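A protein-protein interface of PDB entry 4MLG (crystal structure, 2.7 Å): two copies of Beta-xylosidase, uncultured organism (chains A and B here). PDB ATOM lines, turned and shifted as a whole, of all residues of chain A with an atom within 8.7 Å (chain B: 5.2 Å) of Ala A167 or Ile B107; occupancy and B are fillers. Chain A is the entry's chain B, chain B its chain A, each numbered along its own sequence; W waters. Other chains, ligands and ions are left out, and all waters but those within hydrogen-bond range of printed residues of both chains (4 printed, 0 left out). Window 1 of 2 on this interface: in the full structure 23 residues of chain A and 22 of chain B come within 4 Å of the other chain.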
ATOM      1  N   ASP A 103      15.410  32.045 -25.167  1.00  0.00           N
ATOM      2  CA  ASP A 103      16.193  30.821 -25.036  1.00  0.00           C
ATOM      3  C   ASP A 103      16.870  30.462 -26.355  1.00  0.00           C
ATOM      4  O   ASP A 103      16.874  31.253 -27.298  1.00  0.00           O
ATOM      5  CB  ASP A 103      15.330  29.658 -24.530  1.00  0.00           C
ATOM      6  CG  ASP A 103      14.075  29.444 -25.362  1.00  0.00           C
ATOM      7  OD1 ASP A 103      14.055  29.832 -26.550  1.00  0.00           O
ATOM      8  OD2 ASP A 103      13.102  28.876 -24.823  1.00  0.00           O
ATOM      9  N   ASN A 105      15.828  28.727 -28.487  1.00  0.00           N
ATOM     10  CA  ASN A 105      14.778  28.565 -29.484  1.00  0.00           C
ATOM     11  C   ASN A 105      14.089  29.892 -29.796  1.00  0.00           C
ATOM     12  O   ASN A 105      13.017  29.915 -30.407  1.00  0.00           O
ATOM     13  CB  ASN A 105      13.748  27.542 -29.006  1.00  0.00           C
ATOM     14  CG  ASN A 105      14.366  26.191 -28.705  1.00  0.00           C
ATOM     15  OD1 ASN A 105      14.421  25.763 -27.552  1.00  0.00           O
ATOM     16  ND2 ASN A 105      14.831  25.508 -29.745  1.00  0.00           N
ATOM     17  N   ILE A 107      12.575  31.727 -27.813  1.00  0.00           N
ATOM     18  CA  ILE A 107      11.370  31.867 -27.010  1.00  0.00           C
ATOM     19  C   ILE A 107      11.706  32.617 -25.728  1.00  0.00           C
ATOM     20  O   ILE A 107      12.580  32.198 -24.967  1.00  0.00           O
ATOM     21  CB  ILE A 107      10.772  30.498 -26.648  1.00  0.00           C
ATOM     22  CG1 ILE A 107      10.501  29.684 -27.914  1.00  0.00           C
ATOM     23  CG2 ILE A 107       9.502  30.672 -25.834  1.00  0.00           C
ATOM     24  CD1 ILE A 107       9.930  28.306 -27.643  1.00  0.00           C
ATOM     25  N   PHE A 108      11.016  33.729 -25.491  1.00  0.00           N
ATOM     26  CA  PHE A 108      11.307  34.561 -24.330  1.00  0.00           C
ATOM     27  C   PHE A 108      11.008  33.848 -23.020  1.00  0.00           C
ATOM     28  O   PHE A 108       9.880  33.430 -22.767  1.00  0.00           O
ATOM     29  CB  PHE A 108      10.557  35.893 -24.397  1.00  0.00           C
ATOM     30  CG  PHE A 108      11.442  37.061 -24.724  1.00  0.00           C
ATOM     31  CD1 PHE A 108      12.518  37.377 -23.910  1.00  0.00           C
ATOM     32  CD2 PHE A 108      11.201  37.840 -25.843  1.00  0.00           C
ATOM     33  CE1 PHE A 108      13.340  38.448 -24.207  1.00  0.00           C
ATOM     34  CE2 PHE A 108      12.018  38.914 -26.144  1.00  0.00           C
ATOM     35  CZ  PHE A 108      13.089  39.218 -25.326  1.00  0.00           C
ATOM     36  N   ARG A 109      12.040  33.704 -22.196  1.00  0.00           N
ATOM     37  CA  ARG A 109      11.899  33.119 -20.872  1.00  0.00           C
ATOM     38  C   ARG A 109      12.417  34.115 -19.840  1.00  0.00           C
ATOM     39  O   ARG A 109      13.014  35.130 -20.197  1.00  0.00           O
ATOM     40  CB  ARG A 109      12.688  31.812 -20.774  1.00  0.00           C
ATOM     41  CG  ARG A 109      12.506  30.861 -21.954  1.00  0.00           C
ATOM     42  CD  ARG A 109      11.052  30.446 -22.135  1.00  0.00           C
ATOM     43  NE  ARG A 109      10.446  29.992 -20.886  1.00  0.00           N
ATOM     44  CZ  ARG A 109      10.588  28.770 -20.382  1.00  0.00           C
ATOM     45  NH1 ARG A 109      11.324  27.868 -21.017  1.00  0.00           N
ATOM     46  NH2 ARG A 109       9.995  28.448 -19.241  1.00  0.00           N
ATOM     47  N   GLY A 131       7.732  27.491 -16.564  1.00  0.00           N
ATOM     48  CA  GLY A 131       6.459  28.097 -16.909  1.00  0.00           C
ATOM     49  C   GLY A 131       6.554  29.565 -17.281  1.00  0.00           C
ATOM     50  O   GLY A 131       5.549  30.198 -17.608  1.00  0.00           O
ATOM     51  N   SER A 132       7.763  30.112 -17.233  1.00  0.00           N
ATOM     52  CA  SER A 132       7.971  31.520 -17.549  1.00  0.00           C
ATOM     53  C   SER A 132       7.854  31.791 -19.046  1.00  0.00           C
ATOM     54  O   SER A 132       8.196  30.943 -19.873  1.00  0.00           O
ATOM     55  CB  SER A 132       9.337  31.984 -17.047  1.00  0.00           C
ATOM     56  OG  SER A 132      10.381  31.292 -17.709  1.00  0.00           O
ATOM     57  N   TYR A 133       7.363  32.980 -19.385  1.00  0.00           N
ATOM     58  CA  TYR A 133       7.275  33.416 -20.773  1.00  0.00           C
ATOM     59  C   TYR A 133       7.186  34.937 -20.849  1.00  0.00           C
ATOM     60  O   TYR A 133       7.139  35.613 -19.819  1.00  0.00           O
ATOM     61  CB  TYR A 133       6.086  32.759 -21.487  1.00  0.00           C
ATOM     62  CG  TYR A 133       4.732  33.078 -20.891  1.00  0.00           C
ATOM     63  CD1 TYR A 133       3.905  34.034 -21.467  1.00  0.00           C
ATOM     64  CD2 TYR A 133       4.274  32.414 -19.759  1.00  0.00           C
ATOM     65  CE1 TYR A 133       2.664  34.325 -20.929  1.00  0.00           C
ATOM     66  CE2 TYR A 133       3.036  32.699 -19.214  1.00  0.00           C
ATOM     67  CZ  TYR A 133       2.236  33.655 -19.802  1.00  0.00           C
ATOM     68  OH  TYR A 133       1.004  33.939 -19.260  1.00  0.00           O
ATOM     69  N   GLN A 158       6.080  38.735 -27.190  1.00  0.00           N
ATOM     70  CA  GLN A 158       5.521  37.400 -27.427  1.00  0.00           C
ATOM     71  C   GLN A 158       4.345  37.011 -26.522  1.00  0.00           C
ATOM     72  O   GLN A 158       4.038  35.828 -26.381  1.00  0.00           O
ATOM     73  CB  GLN A 158       6.620  36.331 -27.339  1.00  0.00           C
ATOM     74  CG  GLN A 158       7.791  36.550 -28.286  1.00  0.00           C
ATOM     75  CD  GLN A 158       8.886  35.517 -28.102  1.00  0.00           C
ATOM     76  OE1 GLN A 158       8.946  34.834 -27.080  1.00  0.00           O
ATOM     77  NE2 GLN A 158       9.758  35.394 -29.097  1.00  0.00           N
ATOM     78  N   LEU A 159       3.679  37.994 -25.922  1.00  0.00           N
ATOM     79  CA  LEU A 159       2.567  37.700 -25.019  1.00  0.00           C
ATOM     80  C   LEU A 159       1.382  37.094 -25.765  1.00  0.00           C
ATOM     81  O   LEU A 159       0.690  36.219 -25.245  1.00  0.00           O
ATOM     82  CB  LEU A 159       2.125  38.957 -24.266  1.00  0.00           C
ATOM     83  CG  LEU A 159       1.030  38.790 -23.211  1.00  0.00           C
ATOM     84  CD1 LEU A 159       1.488  37.850 -22.108  1.00  0.00           C
ATOM     85  CD2 LEU A 159       0.626  40.140 -22.637  1.00  0.00           C
ATOM     86  N   GLN A 160       1.164  37.554 -26.992  1.00  0.00           N
ATOM     87  CA  GLN A 160       0.024  37.113 -27.789  1.00  0.00           C
ATOM     88  C   GLN A 160       0.131  35.652 -28.217  1.00  0.00           C
ATOM     89  O   GLN A 160      -0.846  35.062 -28.680  1.00  0.00           O
ATOM     90  CB  GLN A 160      -0.159  38.013 -29.016  1.00  0.00           C
ATOM     91  CG  GLN A 160       0.980  37.957 -30.029  1.00  0.00           C
ATOM     92  CD  GLN A 160       2.204  38.741 -29.592  1.00  0.00           C
ATOM     93  OE1 GLN A 160       2.199  39.398 -28.550  1.00  0.00           O
ATOM     94  NE2 GLN A 160       3.262  38.675 -30.391  1.00  0.00           N
ATOM     95  N   ARG A 161       1.315  35.071 -28.058  1.00  0.00           N
ATOM     96  CA  ARG A 161       1.528  33.670 -28.398  1.00  0.00           C
ATOM     97  C   ARG A 161       0.923  32.747 -27.346  1.00  0.00           C
ATOM     98  O   ARG A 161       0.874  31.531 -27.530  1.00  0.00           O
ATOM     99  CB  ARG A 161       3.021  33.372 -28.527  1.00  0.00           C
ATOM    100  CG  ARG A 161       3.731  34.164 -29.605  1.00  0.00           C
ATOM    101  CD  ARG A 161       5.171  33.709 -29.727  1.00  0.00           C
ATOM    102  NE  ARG A 161       5.885  34.411 -30.787  1.00  0.00           N
ATOM    103  CZ  ARG A 161       7.132  34.133 -31.150  1.00  0.00           C
ATOM    104  NH1 ARG A 161       7.800  33.164 -30.538  1.00  0.00           N
ATOM    105  NH2 ARG A 161       7.710  34.821 -32.124  1.00  0.00           N
ATOM    106  N   TYR A 162       0.465  33.330 -26.244  1.00  0.00           N
ATOM    107  CA  TYR A 162       0.005  32.540 -25.109  1.00  0.00           C
ATOM    108  C   TYR A 162      -1.427  32.865 -24.689  1.00  0.00           C
ATOM    109  O   TYR A 162      -1.860  34.016 -24.742  1.00  0.00           O
ATOM    110  CB  TYR A 162       0.947  32.734 -23.916  1.00  0.00           C
ATOM    111  CG  TYR A 162       2.391  32.383 -24.197  1.00  0.00           C
ATOM    112  CD1 TYR A 162       2.904  31.138 -23.855  1.00  0.00           C
ATOM    113  CD2 TYR A 162       3.244  33.298 -24.802  1.00  0.00           C
ATOM    114  CE1 TYR A 162       4.226  30.815 -24.110  1.00  0.00           C
ATOM    115  CE2 TYR A 162       4.563  32.984 -25.060  1.00  0.00           C
ATOM    116  CZ  TYR A 162       5.049  31.743 -24.713  1.00  0.00           C
ATOM    117  OH  TYR A 162       6.365  31.431 -24.971  1.00  0.00           O
ATOM    118  N   ARG A 163      -2.157  31.834 -24.278  1.00  0.00           N
ATOM    119  CA  ARG A 163      -3.454  32.007 -23.633  1.00  0.00           C
ATOM    120  C   ARG A 163      -3.485  31.126 -22.395  1.00  0.00           C
ATOM    121  O   ARG A 163      -3.313  29.911 -22.492  1.00  0.00           O
ATOM    122  CB  ARG A 163      -4.601  31.632 -24.573  1.00  0.00           C
ATOM    123  CG  ARG A 163      -4.834  32.616 -25.708  1.00  0.00           C
ATOM    124  CD  ARG A 163      -5.090  34.022 -25.187  1.00  0.00           C
ATOM    125  NE  ARG A 163      -5.383  34.960 -26.266  1.00  0.00           N
ATOM    126  CZ  ARG A 163      -4.458  35.557 -27.012  1.00  0.00           C
ATOM    127  NH1 ARG A 163      -3.172  35.312 -26.800  1.00  0.00           N
ATOM    128  NH2 ARG A 163      -4.816  36.397 -27.974  1.00  0.00           N
ATOM    129  N   ASN A 164      -3.700  31.745 -21.236  1.00  0.00           N
ATOM    130  CA  ASN A 164      -3.663  31.040 -19.958  1.00  0.00           C
ATOM    131  C   ASN A 164      -2.352  30.287 -19.774  1.00  0.00           C
ATOM    132  O   ASN A 164      -2.348  29.105 -19.430  1.00  0.00           O
ATOM    133  CB  ASN A 164      -4.852  30.086 -19.821  1.00  0.00           C
ATOM    134  CG  ASN A 164      -6.180  30.788 -19.990  1.00  0.00           C
ATOM    135  OD1 ASN A 164      -6.944  30.484 -20.906  1.00  0.00           O
ATOM    136  ND2 ASN A 164      -6.464  31.738 -19.107  1.00  0.00           N
ATOM    137  N   ASN A 165      -1.250  30.983 -20.042  1.00  0.00           N
ATOM    138  CA  ASN A 165       0.100  30.447 -19.872  1.00  0.00           C
ATOM    139  C   ASN A 165       0.448  29.292 -20.814  1.00  0.00           C
ATOM    140  O   ASN A 165       1.534  28.718 -20.724  1.00  0.00           O
ATOM    141  CB  ASN A 165       0.336  30.047 -18.413  1.00  0.00           C
ATOM    142  CG  ASN A 165      -0.177  31.085 -17.439  1.00  0.00           C
ATOM    143  OD1 ASN A 165      -0.065  32.287 -17.682  1.00  0.00           O
ATOM    144  ND2 ASN A 165      -0.760  30.627 -16.338  1.00  0.00           N
ATOM    145  N   LYS A 166      -0.468  28.959 -21.718  1.00  0.00           N
ATOM    146  CA  LYS A 166      -0.228  27.887 -22.680  1.00  0.00           C
ATOM    147  C   LYS A 166       0.046  28.461 -24.064  1.00  0.00           C
ATOM    148  O   LYS A 166      -0.655  29.364 -24.522  1.00  0.00           O
ATOM    149  CB  LYS A 166      -1.415  26.924 -22.730  1.00  0.00           C
ATOM    150  CG  LYS A 166      -1.824  26.369 -21.376  1.00  0.00           C
ATOM    151  CD  LYS A 166      -0.668  25.665 -20.681  1.00  0.00           C
ATOM    152  CE  LYS A 166      -1.068  25.211 -19.285  1.00  0.00           C
ATOM    153  NZ  LYS A 166       0.050  24.540 -18.567  1.00  0.00           N
ATOM    154  N   ALA A 167       1.072  27.934 -24.725  1.00  0.00           N
ATOM    155  CA  ALA A 167       1.466  28.422 -26.041  1.00  0.00           C
ATOM    156  C   ALA A 167       0.448  28.054 -27.111  1.00  0.00           C
ATOM    157  O   ALA A 167      -0.009  26.914 -27.180  1.00  0.00           O
ATOM    158  CB  ALA A 167       2.836  27.883 -26.413  1.00  0.00           C
ATOM    159  N   LEU A 168       0.098  29.028 -27.944  1.00  0.00           N
ATOM    160  CA  LEU A 168      -0.806  28.793 -29.061  1.00  0.00           C
ATOM    161  C   LEU A 168      -0.031  28.268 -30.263  1.00  0.00           C
ATOM    162  O   LEU A 168       1.166  28.522 -30.397  1.00  0.00           O
ATOM    163  CB  LEU A 168      -1.532  30.083 -29.443  1.00  0.00           C
ATOM    164  CG  LEU A 168      -2.534  30.646 -28.437  1.00  0.00           C
ATOM    165  CD1 LEU A 168      -3.085  31.977 -28.925  1.00  0.00           C
ATOM    166  CD2 LEU A 168      -3.659  29.652 -28.195  1.00  0.00           C
ATOM    167  N   GLU A 169      -0.717  27.534 -31.131  1.00  0.00           N
ATOM    168  CA  GLU A 169      -0.120  27.066 -32.373  1.00  0.00           C
ATOM    169  C   GLU A 169       0.251  28.267 -33.238  1.00  0.00           C
ATOM    170  O   GLU A 169       1.290  28.277 -33.899  1.00  0.00           O
ATOM    171  CB  GLU A 169      -1.097  26.155 -33.120  1.00  0.00           C
ATOM    172  CG  GLU A 169      -0.578  25.620 -34.447  1.00  0.00           C
ATOM    173  CD  GLU A 169       0.400  24.472 -34.282  1.00  0.00           C
ATOM    174  OE1 GLU A 169       0.713  24.107 -33.129  1.00  0.00           O
ATOM    175  OE2 GLU A 169       0.853  23.927 -35.310  1.00  0.00           O
ATOM    176  N   CYS A 170      -0.606  29.281 -33.214  1.00  0.00           N
ATOM    177  CA  CYS A 170      -0.373  30.516 -33.948  1.00  0.00           C
ATOM    178  C   CYS A 170      -0.704  31.707 -33.052  1.00  0.00           C
ATOM    179  O   CYS A 170      -1.707  31.691 -32.340  1.00  0.00           O
ATOM    180  CB  CYS A 170      -1.229  30.552 -35.215  1.00  0.00           C
ATOM    181  SG  CYS A 170      -0.918  31.965 -36.297  1.00  0.00           S
ATOM    182  N   ALA A 171       0.143  32.731 -33.084  1.00  0.00           N
ATOM    183  CA  ALA A 171      -0.055  33.918 -32.254  1.00  0.00           C
ATOM    184  C   ALA A 171      -1.330  34.665 -32.639  1.00  0.00           C
ATOM    185  O   ALA A 171      -1.670  34.758 -33.818  1.00  0.00           O
ATOM    186  CB  ALA A 171       1.151  34.840 -32.348  1.00  0.00           C
ATOM    187  N   LEU B 101       8.186  15.854 -23.468  1.00  0.00           N
ATOM    188  CA  LEU B 101       7.171  16.277 -22.512  1.00  0.00           C
ATOM    189  C   LEU B 101       6.894  17.762 -22.675  1.00  0.00           C
ATOM    190  O   LEU B 101       7.820  18.573 -22.699  1.00  0.00           O
ATOM    191  CB  LEU B 101       7.637  15.992 -21.081  1.00  0.00           C
ATOM    192  CG  LEU B 101       6.674  16.289 -19.930  1.00  0.00           C
ATOM    193  CD1 LEU B 101       5.584  15.233 -19.848  1.00  0.00           C
ATOM    194  CD2 LEU B 101       7.433  16.375 -18.621  1.00  0.00           C
ATOM    195  N   LYS B 102       5.620  18.116 -22.800  1.00  0.00           N
ATOM    196  CA  LYS B 102       5.242  19.518 -22.837  1.00  0.00           C
ATOM    197  C   LYS B 102       5.583  20.137 -21.492  1.00  0.00           C
ATOM    198  O   LYS B 102       5.292  19.557 -20.447  1.00  0.00           O
ATOM    199  CB  LYS B 102       3.748  19.677 -23.125  1.00  0.00           C
ATOM    200  CG  LYS B 102       3.320  19.266 -24.527  1.00  0.00           C
ATOM    201  CD  LYS B 102       1.851  19.594 -24.750  1.00  0.00           C
ATOM    202  CE  LYS B 102       1.399  19.275 -26.166  1.00  0.00           C
ATOM    203  NZ  LYS B 102      -0.046  19.591 -26.343  1.00  0.00           N
ATOM    204  N   ASP B 103       6.217  21.305 -21.514  1.00  0.00           N
ATOM    205  CA  ASP B 103       6.527  22.010 -20.278  1.00  0.00           C
ATOM    206  C   ASP B 103       5.267  22.649 -19.703  1.00  0.00           C
ATOM    207  O   ASP B 103       4.155  22.366 -20.149  1.00  0.00           O
ATOM    208  CB  ASP B 103       7.620  23.061 -20.499  1.00  0.00           C
ATOM    209  CG  ASP B 103       7.308  24.004 -21.649  1.00  0.00           C
ATOM    210  OD1 ASP B 103       6.120  24.162 -22.000  1.00  0.00           O
ATOM    211  OD2 ASP B 103       8.258  24.598 -22.201  1.00  0.00           O
ATOM    212  N   ASN B 105       4.266  25.415 -20.175  1.00  0.00           N
ATOM    213  CA  ASN B 105       3.731  26.330 -21.173  1.00  0.00           C
ATOM    214  C   ASN B 105       3.166  25.564 -22.368  1.00  0.00           C
ATOM    215  O   ASN B 105       2.954  26.136 -23.439  1.00  0.00           O
ATOM    216  CB  ASN B 105       4.813  27.305 -21.640  1.00  0.00           C
ATOM    217  CG  ASN B 105       5.344  28.171 -20.515  1.00  0.00           C
ATOM    218  OD1 ASN B 105       6.523  28.102 -20.166  1.00  0.00           O
ATOM    219  ND2 ASN B 105       4.475  28.998 -19.946  1.00  0.00           N
ATOM    220  N   ASP B 106       2.931  24.269 -22.169  1.00  0.00           N
ATOM    221  CA  ASP B 106       2.455  23.370 -23.223  1.00  0.00           C
ATOM    222  C   ASP B 106       3.348  23.362 -24.465  1.00  0.00           C
ATOM    223  O   ASP B 106       2.871  23.157 -25.581  1.00  0.00           O
ATOM    224  CB  ASP B 106       1.001  23.672 -23.607  1.00  0.00           C
ATOM    225  CG  ASP B 106       0.002  22.835 -22.826  1.00  0.00           C
ATOM    226  OD1 ASP B 106       0.411  21.816 -22.231  1.00  0.00           O
ATOM    227  OD2 ASP B 106      -1.197  23.189 -22.820  1.00  0.00           O
ATOM    228  N   ILE B 107       4.643  23.586 -24.265  1.00  0.00           N
ATOM    229  CA  ILE B 107       5.607  23.501 -25.354  1.00  0.00           C
ATOM    230  C   ILE B 107       6.439  22.234 -25.194  1.00  0.00           C
ATOM    231  O   ILE B 107       7.026  22.003 -24.135  1.00  0.00           O
ATOM    232  CB  ILE B 107       6.539  24.725 -25.382  1.00  0.00           C
ATOM    233  CG1 ILE B 107       5.722  26.015 -25.469  1.00  0.00           C
ATOM    234  CG2 ILE B 107       7.512  24.631 -26.546  1.00  0.00           C
ATOM    235  CD1 ILE B 107       6.563  27.276 -25.503  1.00  0.00           C
ATOM    236  N   PHE B 108       6.486  21.410 -26.239  1.00  0.00           N
ATOM    237  CA  PHE B 108       7.210  20.146 -26.161  1.00  0.00           C
ATOM    238  C   PHE B 108       8.709  20.352 -25.987  1.00  0.00           C
ATOM    239  O   PHE B 108       9.360  21.008 -26.799  1.00  0.00           O
ATOM    240  CB  PHE B 108       6.922  19.257 -27.376  1.00  0.00           C
ATOM    241  CG  PHE B 108       5.974  18.126 -27.084  1.00  0.00           C
ATOM    242  CD1 PHE B 108       6.332  17.114 -26.204  1.00  0.00           C
ATOM    243  CD2 PHE B 108       4.727  18.072 -27.686  1.00  0.00           C
ATOM    244  CE1 PHE B 108       5.462  16.074 -25.926  1.00  0.00           C
ATOM    245  CE2 PHE B 108       3.854  17.032 -27.414  1.00  0.00           C
ATOM    246  CZ  PHE B 108       4.222  16.034 -26.533  1.00  0.00           C
ATOM    247  N   ARG B 109       9.240  19.795 -24.904  1.00  0.00           N
ATOM    248  CA  ARG B 109      10.668  19.832 -24.628  1.00  0.00           C
ATOM    249  C   ARG B 109      11.152  18.404 -24.441  1.00  0.00           C
ATOM    250  O   ARG B 109      10.350  17.469 -24.407  1.00  0.00           O
ATOM    251  CB  ARG B 109      10.956  20.648 -23.367  1.00  0.00           C
ATOM    252  CG  ARG B 109      10.466  22.089 -23.410  1.00  0.00           C
ATOM    253  CD  ARG B 109      11.182  22.895 -24.481  1.00  0.00           C
ATOM    254  NE  ARG B 109      10.948  24.330 -24.334  1.00  0.00           N
ATOM    255  CZ  ARG B 109      11.476  25.258 -25.126  1.00  0.00           C
ATOM    256  NH1 ARG B 109      12.268  24.906 -26.129  1.00  0.00           N
ATOM    257  NH2 ARG B 109      11.210  26.541 -24.917  1.00  0.00           N
ATOM    258  N   GLN B 158       4.594  19.636 -32.908  1.00  0.00           N
ATOM    259  CA  GLN B 158       4.981  21.047 -32.909  1.00  0.00           C
ATOM    260  C   GLN B 158       6.236  21.356 -33.725  1.00  0.00           C
ATOM    261  O   GLN B 158       6.825  22.426 -33.572  1.00  0.00           O
ATOM    262  CB  GLN B 158       5.151  21.563 -31.473  1.00  0.00           C
ATOM    263  CG  GLN B 158       3.931  21.363 -30.590  1.00  0.00           C
ATOM    264  CD  GLN B 158       4.211  21.672 -29.132  1.00  0.00           C
ATOM    265  OE1 GLN B 158       5.355  21.914 -28.746  1.00  0.00           O
ATOM    266  NE2 GLN B 158       3.165  21.666 -28.314  1.00  0.00           N
ATOM    267  N   ARG B 161       6.224  24.525 -35.820  1.00  0.00           N
ATOM    268  CA  ARG B 161       6.312  25.801 -35.121  1.00  0.00           C
ATOM    269  C   ARG B 161       7.718  26.390 -35.209  1.00  0.00           C
ATOM    270  O   ARG B 161       7.932  27.557 -34.876  1.00  0.00           O
ATOM    271  CB  ARG B 161       5.920  25.639 -33.650  1.00  0.00           C
ATOM    272  CG  ARG B 161       4.470  25.248 -33.415  1.00  0.00           C
ATOM    273  CD  ARG B 161       4.186  25.121 -31.926  1.00  0.00           C
ATOM    274  NE  ARG B 161       2.782  24.846 -31.642  1.00  0.00           N
ATOM    275  CZ  ARG B 161       2.285  24.704 -30.417  1.00  0.00           C
ATOM    276  NH1 ARG B 161       3.081  24.812 -29.362  1.00  0.00           N
ATOM    277  NH2 ARG B 161       0.994  24.456 -30.245  1.00  0.00           N
ATOM    278  N   TYR B 162       8.672  25.585 -35.666  1.00  0.00           N
ATOM    279  CA  TYR B 162      10.074  25.989 -35.666  1.00  0.00           C
ATOM    280  C   TYR B 162      10.692  26.010 -37.062  1.00  0.00           C
ATOM    281  O   TYR B 162      10.422  25.139 -37.890  1.00  0.00           O
ATOM    282  CB  TYR B 162      10.893  25.065 -34.756  1.00  0.00           C
ATOM    283  CG  TYR B 162      10.369  24.962 -33.340  1.00  0.00           C
ATOM    284  CD1 TYR B 162      10.857  25.786 -32.334  1.00  0.00           C
ATOM    285  CD2 TYR B 162       9.388  24.037 -33.009  1.00  0.00           C
ATOM    286  CE1 TYR B 162      10.379  25.694 -31.040  1.00  0.00           C
ATOM    287  CE2 TYR B 162       8.905  23.937 -31.718  1.00  0.00           C
ATOM    288  CZ  TYR B 162       9.403  24.767 -30.739  1.00  0.00           C
ATOM    289  OH  TYR B 162       8.923  24.667 -29.454  1.00  0.00           O
HETATM  290  O   HOH W   1       8.107  26.085 -19.080  1.00  0.00           O
HETATM  291  O   HOH W   2       1.444  22.171 -19.779  1.00  0.00           O
HETATM  292  O   HOH W   3       9.226  27.513 -22.834  1.00  0.00           O
HETATM  293  O   HOH W   4       1.291  24.618 -26.923  1.00  0.00           O
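Of the 22 printed residues of chain A, 12 touch a printed residue of chain B. Printed residues of chain A that touch a printed residue of chain B: Asp A103, Asn A105, Ile A107, Arg A109, Gly A131, Ser A132, Tyr A133, Asn A165, Lys A166, Ala A167, Leu A168 and Glu A169. Hydrophobic or aromatic side chains of chain B that line the printed part of chain A: Ile B107. Among the printed residues, 14 pairs touch across the chains.
Among the printed residues, pairs that only touch across the chains: Lys A166 with Asp B106 (3.3 Å), Tyr A133 with Asn B105 (3.4 Å), Ile A107 with Arg B109 (3.5 Å), Ala A167 with Ile B107 (3.6 Å), Arg A109 with Asn B105 (3.6 Å), Lys A166 with Asn B105 (3.7 Å) and Leu A168 with Arg B161 (3.9 Å).
The backbone carbonyl oxygen of Ser A132 lies close to the side-chain amide oxygen of Asn B105, 3.3 Å away. The guanidinium group (NH2) of Arg B109 lies within salt-bridge range of the side-chain carboxylate (OD2) of Asp A103 (3.0 Å). The side-chain amide nitrogen (ND2) of Asn B105 sits at hydrogen-bond distance from the backbone carbonyl oxygen (O) of Asn A165 (3.1 Å). The side-chain amide nitrogen (ND2) of Asn B105 sits at hydrogen-bond distance from the backbone carbonyl oxygen (O) of Gly A131 (2.8 Å). The guanidinium group of Arg B161 is in salt-bridge range of the side-chain carboxylate of Glu A169 (2.7 Å). The guanidinium group (NH1) of Arg B109 is in hydrogen-bond range of the side-chain amide oxygen (OD1) of Asn A105 (2.7 Å). The backbone carbonyl oxygen (O) of Asn B105 lies within hydrogen-bond range of the backbone NH (N) of Ala A167, at 2.9 Å.
The backbone carbonyl oxygen (O) of Asp B106 lies within hydrogen-bond range of the side-chain amide nitrogen (NE2) of Gln B158. O of Ser A132 is in hydrogen-bond range of NE of Arg A109 (2.6 Å). NE of Arg B109 lies within salt-bridge range of OD2 of Asp B103 (3.4 Å). NH1 of Arg B161 sits close to NE2 of Gln B158 (3.3 Å). The backbone carbonyl oxygen of Arg A161 is in hydrogen-bond range of the backbone NH of Leu A168, at 2.7 Å. OD1 of Asn A165 sits at hydrogen-bond distance from OH of Tyr A133.
Asp A103 touches Arg B109, but with the chains exchanged Arg A109 does not touch Asp B103 (4.6 Å). Asn A105 touches Arg B109, and with the chains exchanged Arg A109 touches Asn B105. Ile A107 touches Arg B109, but with the chains exchanged Arg A109 does not touch Ile B107 (6.4 Å). 8 positions are printed for both chains.
Water W4 lies within hydrogen-bond range of the backbone carbonyl oxygen (O) of Asp B106 (2.5 Å), the backbone carbonyl oxygen (O) of Ala A167 (2.7 Å) and the guanidinium group (NH1) of Arg B161 (3.0 Å). Water W2 lies within hydrogen-bond range of OD1 of Asp B106 (2.7 Å), O of Asp B103 (2.7 Å) and NZ of Lys A166 (3.0 Å). Water W1 lies within hydrogen-bond range of OD1 of Asn B105 (2.8 Å), N of Gly A131 (2.9 Å), NH2 of Arg A109 (3.0 Å) and OD2 of Asp B103 (3.5 Å). Water W3 lies within hydrogen-bond range of the guanidinium group of Arg A109, the guanidinium group of Arg B109 and the side-chain carboxylate of Asp B103.
Of chain B, only Asn B105 and Ile B107 come within 4 Å of Ala A167. Ile B107 touches just one residue of chain A: Ala A167. Of the printed residues of chain B, Lys A166 touches Asn B105 (3.7 Å) and Asp B106 (3.3 Å). Of the printed residues of chain A, Asn B105 touches Arg A109 (3.6 Å), Gly A131 (2.8 Å), Ser A132 (3.3 Å), Tyr A133 (3.4 Å), Asn A165 (3.1 Å), Lys A166 (3.7 Å) and Ala A167 (2.9 Å). Cys A170 touches none of the printed residues of chain B. Ala A171 touches none of the printed residues of chain B. The nearest residue of chain B that does not touch Ala A167 is Arg B161 (4.1 Å).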
